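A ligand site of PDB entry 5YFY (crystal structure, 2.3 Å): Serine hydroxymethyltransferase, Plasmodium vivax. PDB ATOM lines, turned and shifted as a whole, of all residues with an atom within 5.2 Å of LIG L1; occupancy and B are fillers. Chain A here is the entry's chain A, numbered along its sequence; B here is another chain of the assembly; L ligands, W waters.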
ATOM      1  N   ILE A  32     -19.714  -2.645  -7.063  1.00  0.00           N
ATOM      2  CA  ILE A  32     -20.321  -1.643  -7.971  1.00  0.00           C
ATOM      3  C   ILE A  32     -19.178  -0.857  -8.606  1.00  0.00           C
ATOM      4  O   ILE A  32     -18.383  -0.277  -7.911  1.00  0.00           O
ATOM      5  CB  ILE A  32     -21.269  -0.627  -7.297  1.00  0.00           C
ATOM      6  CG1 ILE A  32     -22.439  -1.324  -6.558  1.00  0.00           C
ATOM      7  CG2 ILE A  32     -21.820   0.346  -8.321  1.00  0.00           C
ATOM      8  CD1 ILE A  32     -23.426  -2.022  -7.479  1.00  0.00           C
ATOM      9  N   SER A  34     -18.922   1.823 -10.243  1.00  0.00           N
ATOM     10  CA  SER A  34     -18.990   3.281 -10.082  1.00  0.00           C
ATOM     11  C   SER A  34     -18.934   3.776  -8.648  1.00  0.00           C
ATOM     12  O   SER A  34     -19.121   4.961  -8.412  1.00  0.00           O
ATOM     13  CB  SER A  34     -20.310   3.743 -10.693  1.00  0.00           C
ATOM     14  OG  SER A  34     -21.386   3.050 -10.091  1.00  0.00           O
ATOM     15  N   SER A 100     -23.231  17.291 -10.527  1.00  0.00           N
ATOM     16  CA  SER A 100     -23.065  15.865 -10.735  1.00  0.00           C
ATOM     17  C   SER A 100     -22.727  15.561 -12.194  1.00  0.00           C
ATOM     18  O   SER A 100     -22.749  16.454 -13.051  1.00  0.00           O
ATOM     19  CB  SER A 100     -24.351  15.097 -10.343  1.00  0.00           C
ATOM     20  OG  SER A 100     -24.040  13.933  -9.554  1.00  0.00           O
ATOM     21  N   GLY A 101     -22.455  14.296 -12.461  1.00  0.00           N
ATOM     22  CA  GLY A 101     -22.047  13.870 -13.780  1.00  0.00           C
ATOM     23  C   GLY A 101     -23.053  14.181 -14.850  1.00  0.00           C
ATOM     24  O   GLY A 101     -22.692  14.653 -15.925  1.00  0.00           O
ATOM     25  N   SER A 102     -24.324  13.903 -14.559  1.00  0.00           N
ATOM     26  CA  SER A 102     -25.372  14.091 -15.542  1.00  0.00           C
ATOM     27  C   SER A 102     -25.555  15.601 -15.860  1.00  0.00           C
ATOM     28  O   SER A 102     -25.742  15.973 -17.019  1.00  0.00           O
ATOM     29  CB  SER A 102     -26.699  13.464 -15.052  1.00  0.00           C
ATOM     30  OG  SER A 102     -26.572  12.070 -14.745  1.00  0.00           O
ATOM     31  N   ALA A 103     -25.532  16.450 -14.838  1.00  0.00           N
ATOM     32  CA  ALA A 103     -25.596  17.904 -15.022  1.00  0.00           C
ATOM     33  C   ALA A 103     -24.447  18.429 -15.937  1.00  0.00           C
ATOM     34  O   ALA A 103     -24.683  19.084 -16.929  1.00  0.00           O
ATOM     35  CB  ALA A 103     -25.593  18.607 -13.663  1.00  0.00           C
ATOM     36  N   ASN A 105     -22.656  16.788 -18.180  1.00  0.00           N
ATOM     37  CA  ASN A 105     -22.839  16.403 -19.582  1.00  0.00           C
ATOM     38  C   ASN A 105     -23.915  17.238 -20.325  1.00  0.00           C
ATOM     39  O   ASN A 105     -23.702  17.624 -21.477  1.00  0.00           O
ATOM     40  CB  ASN A 105     -23.171  14.914 -19.733  1.00  0.00           C
ATOM     41  CG  ASN A 105     -21.967  14.004 -19.481  1.00  0.00           C
ATOM     42  OD1 ASN A 105     -20.843  14.440 -19.216  1.00  0.00           O
ATOM     43  ND2 ASN A 105     -22.216  12.698 -19.584  1.00  0.00           N
ATOM     44  N   HIS A 129     -23.824   6.013 -21.388  1.00  0.00           N
ATOM     45  CA  HIS A 129     -24.629   6.611 -20.319  1.00  0.00           C
ATOM     46  C   HIS A 129     -25.941   7.167 -20.838  1.00  0.00           C
ATOM     47  O   HIS A 129     -26.109   7.391 -22.035  1.00  0.00           O
ATOM     48  CB  HIS A 129     -23.855   7.703 -19.571  1.00  0.00           C
ATOM     49  CG  HIS A 129     -24.463   8.075 -18.250  1.00  0.00           C
ATOM     50  ND1 HIS A 129     -24.995   9.317 -18.006  1.00  0.00           N
ATOM     51  CD2 HIS A 129     -24.692   7.345 -17.128  1.00  0.00           C
ATOM     52  CE1 HIS A 129     -25.512   9.353 -16.785  1.00  0.00           C
ATOM     53  NE2 HIS A 129     -25.320   8.170 -16.233  1.00  0.00           N
ATOM     54  N   THR A 131     -27.104  10.185 -20.313  1.00  0.00           N
ATOM     55  CA  THR A 131     -26.816  11.534 -20.817  1.00  0.00           C
ATOM     56  C   THR A 131     -26.048  11.595 -22.142  1.00  0.00           C
ATOM     57  O   THR A 131     -25.655  12.686 -22.564  1.00  0.00           O
ATOM     58  CB  THR A 131     -26.040  12.329 -19.755  1.00  0.00           C
ATOM     59  OG1 THR A 131     -24.842  11.626 -19.394  1.00  0.00           O
ATOM     60  CG2 THR A 131     -26.928  12.525 -18.524  1.00  0.00           C
ATOM     61  N   HIS A 132     -25.833  10.444 -22.807  1.00  0.00           N
ATOM     62  CA  HIS A 132     -25.225  10.409 -24.126  1.00  0.00           C
ATOM     63  C   HIS A 132     -26.276  10.280 -25.239  1.00  0.00           C
ATOM     64  O   HIS A 132     -25.991   9.755 -26.307  1.00  0.00           O
ATOM     65  CB  HIS A 132     -24.205   9.262 -24.208  1.00  0.00           C
ATOM     66  CG  HIS A 132     -23.099   9.368 -23.195  1.00  0.00           C
ATOM     67  ND1 HIS A 132     -22.142   8.386 -23.041  1.00  0.00           N
ATOM     68  CD2 HIS A 132     -22.802  10.328 -22.293  1.00  0.00           C
ATOM     69  CE1 HIS A 132     -21.290   8.744 -22.096  1.00  0.00           C
ATOM     70  NE2 HIS A 132     -21.670   9.923 -21.630  1.00  0.00           N
ATOM     71  N   GLY A 181     -16.304   7.480 -24.327  1.00  0.00           N
ATOM     72  CA  GLY A 181     -16.141   7.307 -22.856  1.00  0.00           C
ATOM     73  C   GLY A 181     -17.487   6.817 -22.295  1.00  0.00           C
ATOM     74  O   GLY A 181     -18.537   7.388 -22.630  1.00  0.00           O
ATOM     75  N   TYR A 182     -17.468   5.751 -21.491  1.00  0.00           N
ATOM     76  CA  TYR A 182     -18.695   4.962 -21.235  1.00  0.00           C
ATOM     77  C   TYR A 182     -18.963   4.565 -19.785  1.00  0.00           C
ATOM     78  O   TYR A 182     -18.161   4.827 -18.909  1.00  0.00           O
ATOM     79  CB  TYR A 182     -18.659   3.734 -22.132  1.00  0.00           C
ATOM     80  CG  TYR A 182     -18.265   4.050 -23.568  1.00  0.00           C
ATOM     81  CD1 TYR A 182     -19.123   4.778 -24.413  1.00  0.00           C
ATOM     82  CD2 TYR A 182     -17.031   3.641 -24.089  1.00  0.00           C
ATOM     83  CE1 TYR A 182     -18.766   5.076 -25.735  1.00  0.00           C
ATOM     84  CE2 TYR A 182     -16.670   3.929 -25.415  1.00  0.00           C
ATOM     85  CZ  TYR A 182     -17.549   4.640 -26.230  1.00  0.00           C
ATOM     86  OH  TYR A 182     -17.205   4.920 -27.518  1.00  0.00           O
ATOM     87  N   THR A 183     -20.129   3.982 -19.537  1.00  0.00           N
ATOM     88  CA  THR A 183     -20.487   3.561 -18.181  1.00  0.00           C
ATOM     89  C   THR A 183     -20.131   2.122 -17.915  1.00  0.00           C
ATOM     90  O   THR A 183     -19.718   1.803 -16.822  1.00  0.00           O
ATOM     91  CB  THR A 183     -21.955   3.828 -17.765  1.00  0.00           C
ATOM     92  OG1 THR A 183     -22.723   2.613 -17.758  1.00  0.00           O
ATOM     93  CG2 THR A 183     -22.586   4.828 -18.595  1.00  0.00           C
ATOM     94  N   ASP A 208     -16.270  11.367 -22.101  1.00  0.00           N
ATOM     95  CA  ASP A 208     -16.763  11.225 -20.725  1.00  0.00           C
ATOM     96  C   ASP A 208     -15.964  10.104 -20.109  1.00  0.00           C
ATOM     97  O   ASP A 208     -16.220   8.951 -20.370  1.00  0.00           O
ATOM     98  CB  ASP A 208     -18.268  10.898 -20.715  1.00  0.00           C
ATOM     99  CG  ASP A 208     -18.874  10.854 -19.291  1.00  0.00           C
ATOM    100  OD1 ASP A 208     -18.151  10.812 -18.272  1.00  0.00           O
ATOM    101  OD2 ASP A 208     -20.128  10.861 -19.225  1.00  0.00           O
ATOM    102  N   SER A 210     -15.537   9.532 -16.695  1.00  0.00           N
ATOM    103  CA  SER A 210     -15.950   9.352 -15.285  1.00  0.00           C
ATOM    104  C   SER A 210     -15.545   8.015 -14.674  1.00  0.00           C
ATOM    105  O   SER A 210     -15.089   7.992 -13.546  1.00  0.00           O
ATOM    106  CB  SER A 210     -17.461   9.457 -15.165  1.00  0.00           C
ATOM    107  OG  SER A 210     -17.905  10.743 -15.574  1.00  0.00           O
ATOM    108  N   HIS A 211     -15.694   6.948 -15.425  1.00  0.00           N
ATOM    109  CA  HIS A 211     -15.311   5.597 -14.961  1.00  0.00           C
ATOM    110  C   HIS A 211     -13.806   5.329 -14.938  1.00  0.00           C
ATOM    111  O   HIS A 211     -13.356   4.521 -14.148  1.00  0.00           O
ATOM    112  CB  HIS A 211     -16.034   4.519 -15.760  1.00  0.00           C
ATOM    113  CG  HIS A 211     -17.316   4.091 -15.143  1.00  0.00           C
ATOM    114  ND1 HIS A 211     -17.381   3.136 -14.166  1.00  0.00           N
ATOM    115  CD2 HIS A 211     -18.583   4.529 -15.331  1.00  0.00           C
ATOM    116  CE1 HIS A 211     -18.635   2.962 -13.799  1.00  0.00           C
ATOM    117  NE2 HIS A 211     -19.386   3.799 -14.485  1.00  0.00           N
ATOM    118  N   THR A 234     -17.028  12.724 -13.571  1.00  0.00           N
ATOM    119  CA  THR A 234     -17.447  12.740 -12.182  1.00  0.00           C
ATOM    120  C   THR A 234     -16.223  12.663 -11.292  1.00  0.00           C
ATOM    121  O   THR A 234     -15.194  12.160 -11.701  1.00  0.00           O
ATOM    122  CB  THR A 234     -18.415  11.579 -11.830  1.00  0.00           C
ATOM    123  OG1 THR A 234     -17.795  10.312 -12.069  1.00  0.00           O
ATOM    124  CG2 THR A 234     -19.676  11.690 -12.629  1.00  0.00           C
ATOM    125  N   HIS A 236     -16.537  11.206  -8.145  1.00  0.00           N
ATOM    126  CA  HIS A 236     -16.928  10.242  -7.077  1.00  0.00           C
ATOM    127  C   HIS A 236     -16.701   8.768  -7.340  1.00  0.00           C
ATOM    128  O   HIS A 236     -16.886   7.981  -6.429  1.00  0.00           O
ATOM    129  CB  HIS A 236     -18.392  10.400  -6.602  1.00  0.00           C
ATOM    130  CG  HIS A 236     -19.397  10.477  -7.705  1.00  0.00           C
ATOM    131  ND1 HIS A 236     -19.679  11.653  -8.369  1.00  0.00           N
ATOM    132  CD2 HIS A 236     -20.225   9.545  -8.229  1.00  0.00           C
ATOM    133  CE1 HIS A 236     -20.623  11.435  -9.266  1.00  0.00           C
ATOM    134  NE2 HIS A 236     -20.964  10.162  -9.208  1.00  0.00           N
ATOM    135  N   LYS A 237     -16.294   8.388  -8.535  1.00  0.00           N
ATOM    136  CA  LYS A 237     -16.073   6.967  -8.797  1.00  0.00           C
ATOM    137  C   LYS A 237     -14.603   6.616  -8.506  1.00  0.00           C
ATOM    138  O   LYS A 237     -14.154   6.747  -7.343  1.00  0.00           O
ATOM    139  CB  LYS A 237     -16.482   6.646 -10.212  1.00  0.00           C
ATOM    140  CG  LYS A 237     -17.883   7.063 -10.551  1.00  0.00           C
ATOM    141  CD  LYS A 237     -18.162   6.771 -12.006  1.00  0.00           C
ATOM    142  CE  LYS A 237     -19.606   7.074 -12.323  1.00  0.00           C
ATOM    143  NZ  LYS A 237     -19.900   8.496 -12.113  1.00  0.00           N
ATOM    144  N   ARG A 243     -19.392  13.587  -4.491  1.00  0.00           N
ATOM    145  CA  ARG A 243     -20.313  13.582  -5.625  1.00  0.00           C
ATOM    146  C   ARG A 243     -20.327  14.984  -6.287  1.00  0.00           C
ATOM    147  O   ARG A 243     -20.892  15.898  -5.745  1.00  0.00           O
ATOM    148  CB  ARG A 243     -21.717  13.126  -5.223  1.00  0.00           C
ATOM    149  CG  ARG A 243     -21.711  11.741  -4.584  1.00  0.00           C
ATOM    150  CD  ARG A 243     -23.112  11.198  -4.288  1.00  0.00           C
ATOM    151  NE  ARG A 243     -23.589  10.395  -5.388  1.00  0.00           N
ATOM    152  CZ  ARG A 243     -23.225   9.150  -5.645  1.00  0.00           C
ATOM    153  NH1 ARG A 243     -22.357   8.495  -4.872  1.00  0.00           N
ATOM    154  NH2 ARG A 243     -23.714   8.549  -6.726  1.00  0.00           N
ATOM    155  N   ARG A 371     -22.247  -6.396 -14.051  1.00  0.00           N
ATOM    156  CA  ARG A 371     -21.063  -5.615 -14.039  1.00  0.00           C
ATOM    157  C   ARG A 371     -20.446  -5.622 -12.649  1.00  0.00           C
ATOM    158  O   ARG A 371     -21.133  -5.420 -11.641  1.00  0.00           O
ATOM    159  CB  ARG A 371     -21.388  -4.191 -14.457  1.00  0.00           C
ATOM    160  CG  ARG A 371     -20.175  -3.296 -14.644  1.00  0.00           C
ATOM    161  CD  ARG A 371     -20.633  -1.892 -14.922  1.00  0.00           C
ATOM    162  NE  ARG A 371     -21.223  -1.310 -13.734  1.00  0.00           N
ATOM    163  CZ  ARG A 371     -21.561  -0.038 -13.594  1.00  0.00           C
ATOM    164  NH1 ARG A 371     -21.367   0.840 -14.594  1.00  0.00           N
ATOM    165  NH2 ARG A 371     -22.075   0.350 -12.443  1.00  0.00           N
ATOM    166  N   TYR B  54     -24.525   4.585  -4.710  1.00  0.00           N
ATOM    167  CA  TYR B  54     -25.310   4.755  -5.942  1.00  0.00           C
ATOM    168  C   TYR B  54     -26.722   4.179  -5.757  1.00  0.00           C
ATOM    169  O   TYR B  54     -26.880   3.006  -5.492  1.00  0.00           O
ATOM    170  CB  TYR B  54     -24.634   4.147  -7.221  1.00  0.00           C
ATOM    171  CG  TYR B  54     -24.131   5.237  -8.172  1.00  0.00           C
ATOM    172  CD1 TYR B  54     -25.028   6.015  -8.876  1.00  0.00           C
ATOM    173  CD2 TYR B  54     -22.764   5.539  -8.295  1.00  0.00           C
ATOM    174  CE1 TYR B  54     -24.605   7.042  -9.702  1.00  0.00           C
ATOM    175  CE2 TYR B  54     -22.314   6.578  -9.123  1.00  0.00           C
ATOM    176  CZ  TYR B  54     -23.239   7.331  -9.821  1.00  0.00           C
ATOM    177  OH  TYR B  54     -22.825   8.364 -10.636  1.00  0.00           O
ATOM    178  N   GLU B  56     -29.706   5.074  -8.030  1.00  0.00           N
ATOM    179  CA  GLU B  56     -30.535   5.567  -9.137  1.00  0.00           C
ATOM    180  C   GLU B  56     -31.928   4.965  -9.119  1.00  0.00           C
ATOM    181  O   GLU B  56     -32.089   3.777  -8.879  1.00  0.00           O
ATOM    182  CB  GLU B  56     -29.880   5.259 -10.494  1.00  0.00           C
ATOM    183  CG  GLU B  56     -28.624   6.078 -10.807  1.00  0.00           C
ATOM    184  CD  GLU B  56     -27.955   5.617 -12.097  1.00  0.00           C
ATOM    185  OE1 GLU B  56     -27.261   4.580 -12.071  1.00  0.00           O
ATOM    186  OE2 GLU B  56     -28.133   6.251 -13.158  1.00  0.00           O
ATOM    187  N   TYR B  64     -30.359  -0.802  -8.318  1.00  0.00           N
ATOM    188  CA  TYR B  64     -29.418  -1.642  -7.580  1.00  0.00           C
ATOM    189  C   TYR B  64     -29.996  -2.158  -6.288  1.00  0.00           C
ATOM    190  O   TYR B  64     -31.007  -1.664  -5.802  1.00  0.00           O
ATOM    191  CB  TYR B  64     -28.166  -0.848  -7.235  1.00  0.00           C
ATOM    192  CG  TYR B  64     -27.431  -0.261  -8.397  1.00  0.00           C
ATOM    193  CD1 TYR B  64     -27.771  -0.563  -9.724  1.00  0.00           C
ATOM    194  CD2 TYR B  64     -26.345   0.579  -8.172  1.00  0.00           C
ATOM    195  CE1 TYR B  64     -27.057  -0.012 -10.771  1.00  0.00           C
ATOM    196  CE2 TYR B  64     -25.623   1.131  -9.213  1.00  0.00           C
ATOM    197  CZ  TYR B  64     -25.974   0.844 -10.497  1.00  0.00           C
ATOM    198  OH  TYR B  64     -25.244   1.421 -11.504  1.00  0.00           O
ATOM    199  N   GLN B 270     -31.254  14.022 -13.952  1.00  0.00           N
ATOM    200  CA  GLN B 270     -30.223  13.584 -13.011  1.00  0.00           C
ATOM    201  C   GLN B 270     -29.871  12.112 -13.141  1.00  0.00           C
ATOM    202  O   GLN B 270     -30.575  11.374 -13.799  1.00  0.00           O
ATOM    203  CB  GLN B 270     -30.656  13.871 -11.575  1.00  0.00           C
ATOM    204  CG  GLN B 270     -30.997  15.348 -11.379  1.00  0.00           C
ATOM    205  CD  GLN B 270     -31.182  15.760  -9.936  1.00  0.00           C
ATOM    206  OE1 GLN B 270     -31.136  16.956  -9.607  1.00  0.00           O
ATOM    207  NE2 GLN B 270     -31.377  14.787  -9.050  1.00  0.00           N
ATOM    208  N   GLY B 271     -28.749  11.721 -12.532  1.00  0.00           N
ATOM    209  CA  GLY B 271     -28.375  10.333 -12.360  1.00  0.00           C
ATOM    210  C   GLY B 271     -28.574   9.937 -10.901  1.00  0.00           C
ATOM    211  O   GLY B 271     -29.672  10.038 -10.348  1.00  0.00           O
ATOM    212  N   GLY B 272     -27.501   9.499 -10.274  1.00  0.00           N
ATOM    213  CA  GLY B 272     -27.564   9.060  -8.867  1.00  0.00           C
ATOM    214  C   GLY B 272     -27.930  10.187  -7.941  1.00  0.00           C
ATOM    215  O   GLY B 272     -27.381  11.272  -8.075  1.00  0.00           O
ATOM    216  N   HIS B 274     -27.974  12.331  -4.419  1.00  0.00           N
ATOM    217  CA  HIS B 274     -26.986  12.564  -3.385  1.00  0.00           C
ATOM    218  C   HIS B 274     -27.646  12.296  -2.055  1.00  0.00           C
ATOM    219  O   HIS B 274     -28.408  13.123  -1.543  1.00  0.00           O
ATOM    220  CB  HIS B 274     -26.441  13.970  -3.476  1.00  0.00           C
ATOM    221  CG  HIS B 274     -25.655  14.247  -4.724  1.00  0.00           C
ATOM    222  ND1 HIS B 274     -24.772  15.295  -4.806  1.00  0.00           N
ATOM    223  CD2 HIS B 274     -25.601  13.623  -5.923  1.00  0.00           C
ATOM    224  CE1 HIS B 274     -24.224  15.320  -6.008  1.00  0.00           C
ATOM    225  NE2 HIS B 274     -24.716  14.317  -6.705  1.00  0.00           N
HETATM  226  N1  LIG L   1     -21.117   9.664 -17.024  1.00  0.00           N
HETATM  227  C1  LIG L   1     -20.843   8.361 -16.982  1.00  0.00           C
HETATM  228  C2  LIG L   1     -19.929   7.780 -18.045  1.00  0.00           C
HETATM  229  C3  LIG L   1     -21.407   7.507 -15.903  1.00  0.00           C
HETATM  230  O1  LIG L   1     -21.150   6.189 -15.869  1.00  0.00           O
HETATM  231  C4  LIG L   1     -22.296   8.144 -14.911  1.00  0.00           C
HETATM  232  C5  LIG L   1     -22.904   7.336 -13.752  1.00  0.00           C
HETATM  233  C6  LIG L   1     -22.497   9.616 -15.071  1.00  0.00           C
HETATM  234  C7  LIG L   1     -21.908  10.279 -16.154  1.00  0.00           C
HETATM  235  C8  LIG L   1     -23.405  10.460 -14.213  1.00  0.00           C
HETATM  236  O2  LIG L   1     -23.039  10.667 -12.872  1.00  0.00           O
HETATM  237  P1  LIG L   1     -24.201  11.169 -11.856  1.00  0.00           P
HETATM  238  O3  LIG L   1     -25.150  12.079 -12.544  1.00  0.00           O
HETATM  239  O4  LIG L   1     -24.836   9.864 -11.437  1.00  0.00           O
HETATM  240  O5  LIG L   1     -23.272  11.800 -10.867  1.00  0.00           O
HETATM  241  C9  LIG L   1     -22.821   3.871 -12.892  1.00  0.00           C
HETATM  242  O6  LIG L   1     -23.021   3.042 -12.004  1.00  0.00           O
HETATM  243  O7  LIG L   1     -21.906   3.729 -13.726  1.00  0.00           O
HETATM  244  C10 LIG L   1     -23.700   5.097 -12.950  1.00  0.00           C
HETATM  245  N2  LIG L   1     -23.325   5.982 -14.035  1.00  0.00           N
HETATM  246  C1  LG2 L   2     -25.649   1.699 -18.555  1.00  0.00           C
HETATM  247  C2  LG2 L   2     -26.287   0.693 -17.898  1.00  0.00           C
HETATM  248  C3  LG2 L   2     -26.988   0.926 -16.537  1.00  0.00           C
HETATM  249  C4  LG2 L   2     -27.081   2.386 -16.215  1.00  0.00           C
HETATM  250  C5  LG2 L   2     -26.376   3.415 -16.960  1.00  0.00           C
HETATM  251  C6  LG2 L   2     -27.806   3.193 -15.178  1.00  0.00           C
HETATM  252  C7  LG2 L   2     -26.088   0.276 -15.449  1.00  0.00           C
HETATM  253  C8  LG2 L   2     -26.760   0.121 -14.071  1.00  0.00           C
HETATM  254  C9  LG2 L   2     -28.657  -1.016 -16.387  1.00  0.00           C
HETATM  255  C10 LG2 L   2     -29.933  -1.553 -16.494  1.00  0.00           C
HETATM  256  C11 LG2 L   2     -30.847   0.608 -17.157  1.00  0.00           C
HETATM  257  N1  LG2 L   2     -31.906   1.465 -17.585  1.00  0.00           N
HETATM  258  C12 LG2 L   2     -31.924   2.843 -17.038  1.00  0.00           C
HETATM  259  C13 LG2 L   2     -33.346   3.437 -17.132  1.00  0.00           C
HETATM  260  O1  LG2 L   2     -35.889   3.666 -19.759  1.00  0.00           O
HETATM  261  C14 LG2 L   2     -35.322   3.745 -18.640  1.00  0.00           C
HETATM  262  O2  LG2 L   2     -35.882   4.322 -17.668  1.00  0.00           O
HETATM  263  C15 LG2 L   2     -33.957   3.097 -18.483  1.00  0.00           C
HETATM  264  C16 LG2 L   2     -34.145   1.602 -18.589  1.00  0.00           C
HETATM  265  C17 LG2 L   2     -32.780   0.928 -18.655  1.00  0.00           C
HETATM  266  C18 LG2 L   2     -31.032  -0.759 -16.879  1.00  0.00           C
HETATM  267  F1  LG2 L   2     -30.077  -2.855 -16.228  1.00  0.00           F
HETATM  268  C19 LG2 L   2     -29.540   1.124 -17.055  1.00  0.00           C
HETATM  269  C20 LG2 L   2     -28.416   0.347 -16.655  1.00  0.00           C
HETATM  270  C21 LG2 L   2     -24.705   0.929 -15.235  1.00  0.00           C
HETATM  271  C22 LG2 L   2     -26.367  -0.498 -18.345  1.00  0.00           C
HETATM  272  N2  LG2 L   2     -26.438  -1.610 -18.751  1.00  0.00           N
HETATM  273  N3  LG2 L   2     -25.035   1.533 -19.717  1.00  0.00           N
HETATM  274  C23 LG2 L   2     -28.752   2.731 -14.092  1.00  0.00           C
HETATM  275  N4  LG2 L   2     -27.464   4.483 -15.418  1.00  0.00           N
HETATM  276  N5  LG2 L   2     -26.586   4.662 -16.509  1.00  0.00           N
HETATM  277  O3  LG2 L   2     -25.572   3.053 -17.996  1.00  0.00           O
HETATM  278  O   HOH W   1     -24.241  10.969  -8.273  1.00  0.00           O
HETATM  279  O   HOH W   2     -27.163  13.368 -10.637  1.00  0.00           O
HETATM  280  O   HOH W   3     -26.053   8.139 -13.417  1.00  0.00           O
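The side-chain hydroxyl (OG) of Ser 34 lies within hydrogen-bond range of an oxygen (O6) of LIG L1 (2.5 Å).
The backbone NH (N) of Ser 102 lies within hydrogen-bond range of an oxygen (O3) of LIG L1 (2.8 Å).
OG of Ser 102 is in hydrogen-bond range of O3 of LIG L1 (2.6 Å).
The side-chain hydroxyl (OG) of Ser 100 is in hydrogen-bond range of an oxygen (O5) of LIG L1, at 2.6 Å.
An oxygen (O7) of LIG L1 sits at hydrogen-bond distance from a ring nitrogen (NE2) of His 211 (2.6 Å).
OH of Tyr 54 of chain B lies within hydrogen-bond range of O4 of LIG L1 (2.6 Å).
The side-chain carboxylate (OD2) of Asp 208 is in hydrogen-bond range of a nitrogen (N1) of LIG L1, 2.7 Å away.
An oxygen (O6) of LIG L1 sits at hydrogen-bond distance from the side-chain hydroxyl (OH) of Tyr 64 of chain B (2.8 Å).
An oxygen (O6) of LIG L1 lies within salt-bridge range of the guanidinium group of Arg 371 (2.9 Å).
An oxygen (O4) of LIG L1 lies within hydrogen-bond range of the backbone NH (N) of Gly 272 of chain B.
The backbone NH (N) of Gly 101 sits at hydrogen-bond distance from an oxygen (O5) of LIG L1 (3.1 Å).
A ring nitrogen (NE2) of His 236 lies close to an oxygen (O5) of LIG L1 (3.3 Å).
O3 of LG2 L2 lies within hydrogen-bond range of OG1 of Thr 183, at 2.9 Å.
N4 of LG2 L2 is in hydrogen-bond range of OE2 of Glu 56 of chain B.
OG of Ser 100 is in hydrogen-bond range of NE2 of His 274 of chain B.
NE2 of His 211 lies within hydrogen-bond range of O of Thr 183 (3.1 Å).
OD1 of Asp 208 lies within hydrogen-bond range of OG of Ser 210 (2.7 Å).
The side-chain amide nitrogen (ND2) of Asn 105 sits at hydrogen-bond distance from the side-chain carboxylate (OD2) of Asp 208, 2.8 Å away.
O of Thr 183 is in hydrogen-bond range of NH1 of Arg 371 (2.9 Å).
A ring nitrogen (ND1) of His 132 lies within hydrogen-bond range of the backbone NH of His 129 (3.3 Å).
OG1 of Thr 234 lies within hydrogen-bond range of NZ of Lys 237 (2.8 Å).
The side-chain hydroxyl (OG) of Ser 210 sits at hydrogen-bond distance from the backbone NH (N) of Thr 234 (3.0 Å).
Residues that only touch LIG L1: His 129 (3.3 Å), Tyr 182 (3.5 Å), Thr 183 (3.1 Å), Ser 210 (3.7 Å), Thr 234 (3.5 Å), Lys 237 (3.6 Å), Glu 56 of chain B (3.7 Å) and Gly 271 of chain B (3.6 Å).
Hydrophobic or aromatic side chains within 4 Å of LIG L1: His 129, His 211, His 236, Tyr 54 of chain B and Tyr 64 of chain B.
Of the 28 residues printed, 19 come within 4 Å of LIG L1.
Along chain A the residues within 4 Å of LIG L1 span positions 34 to 371.
The nearest printed residue that does not touch LIG L1 is Asn 105 (4.1 Å).
Water W1 lies within hydrogen-bond range of O5 of LIG L1, NH2 of Arg 243, O of Gly 272 of chain B and OG of Ser 100.
Water W3 lies within hydrogen-bond range of OE2 of Glu 56 of chain B (2.8 Å), O4 of LIG L1 (2.9 Å) and NE2 of His 129 (2.9 Å).
Water W2 lies within hydrogen-bond range of the backbone NH of Gly 271 of chain B, an oxygen (O3) of LIG L1, the backbone carbonyl oxygen of Gly 272 of chain B and the side-chain hydroxyl of Ser 100.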
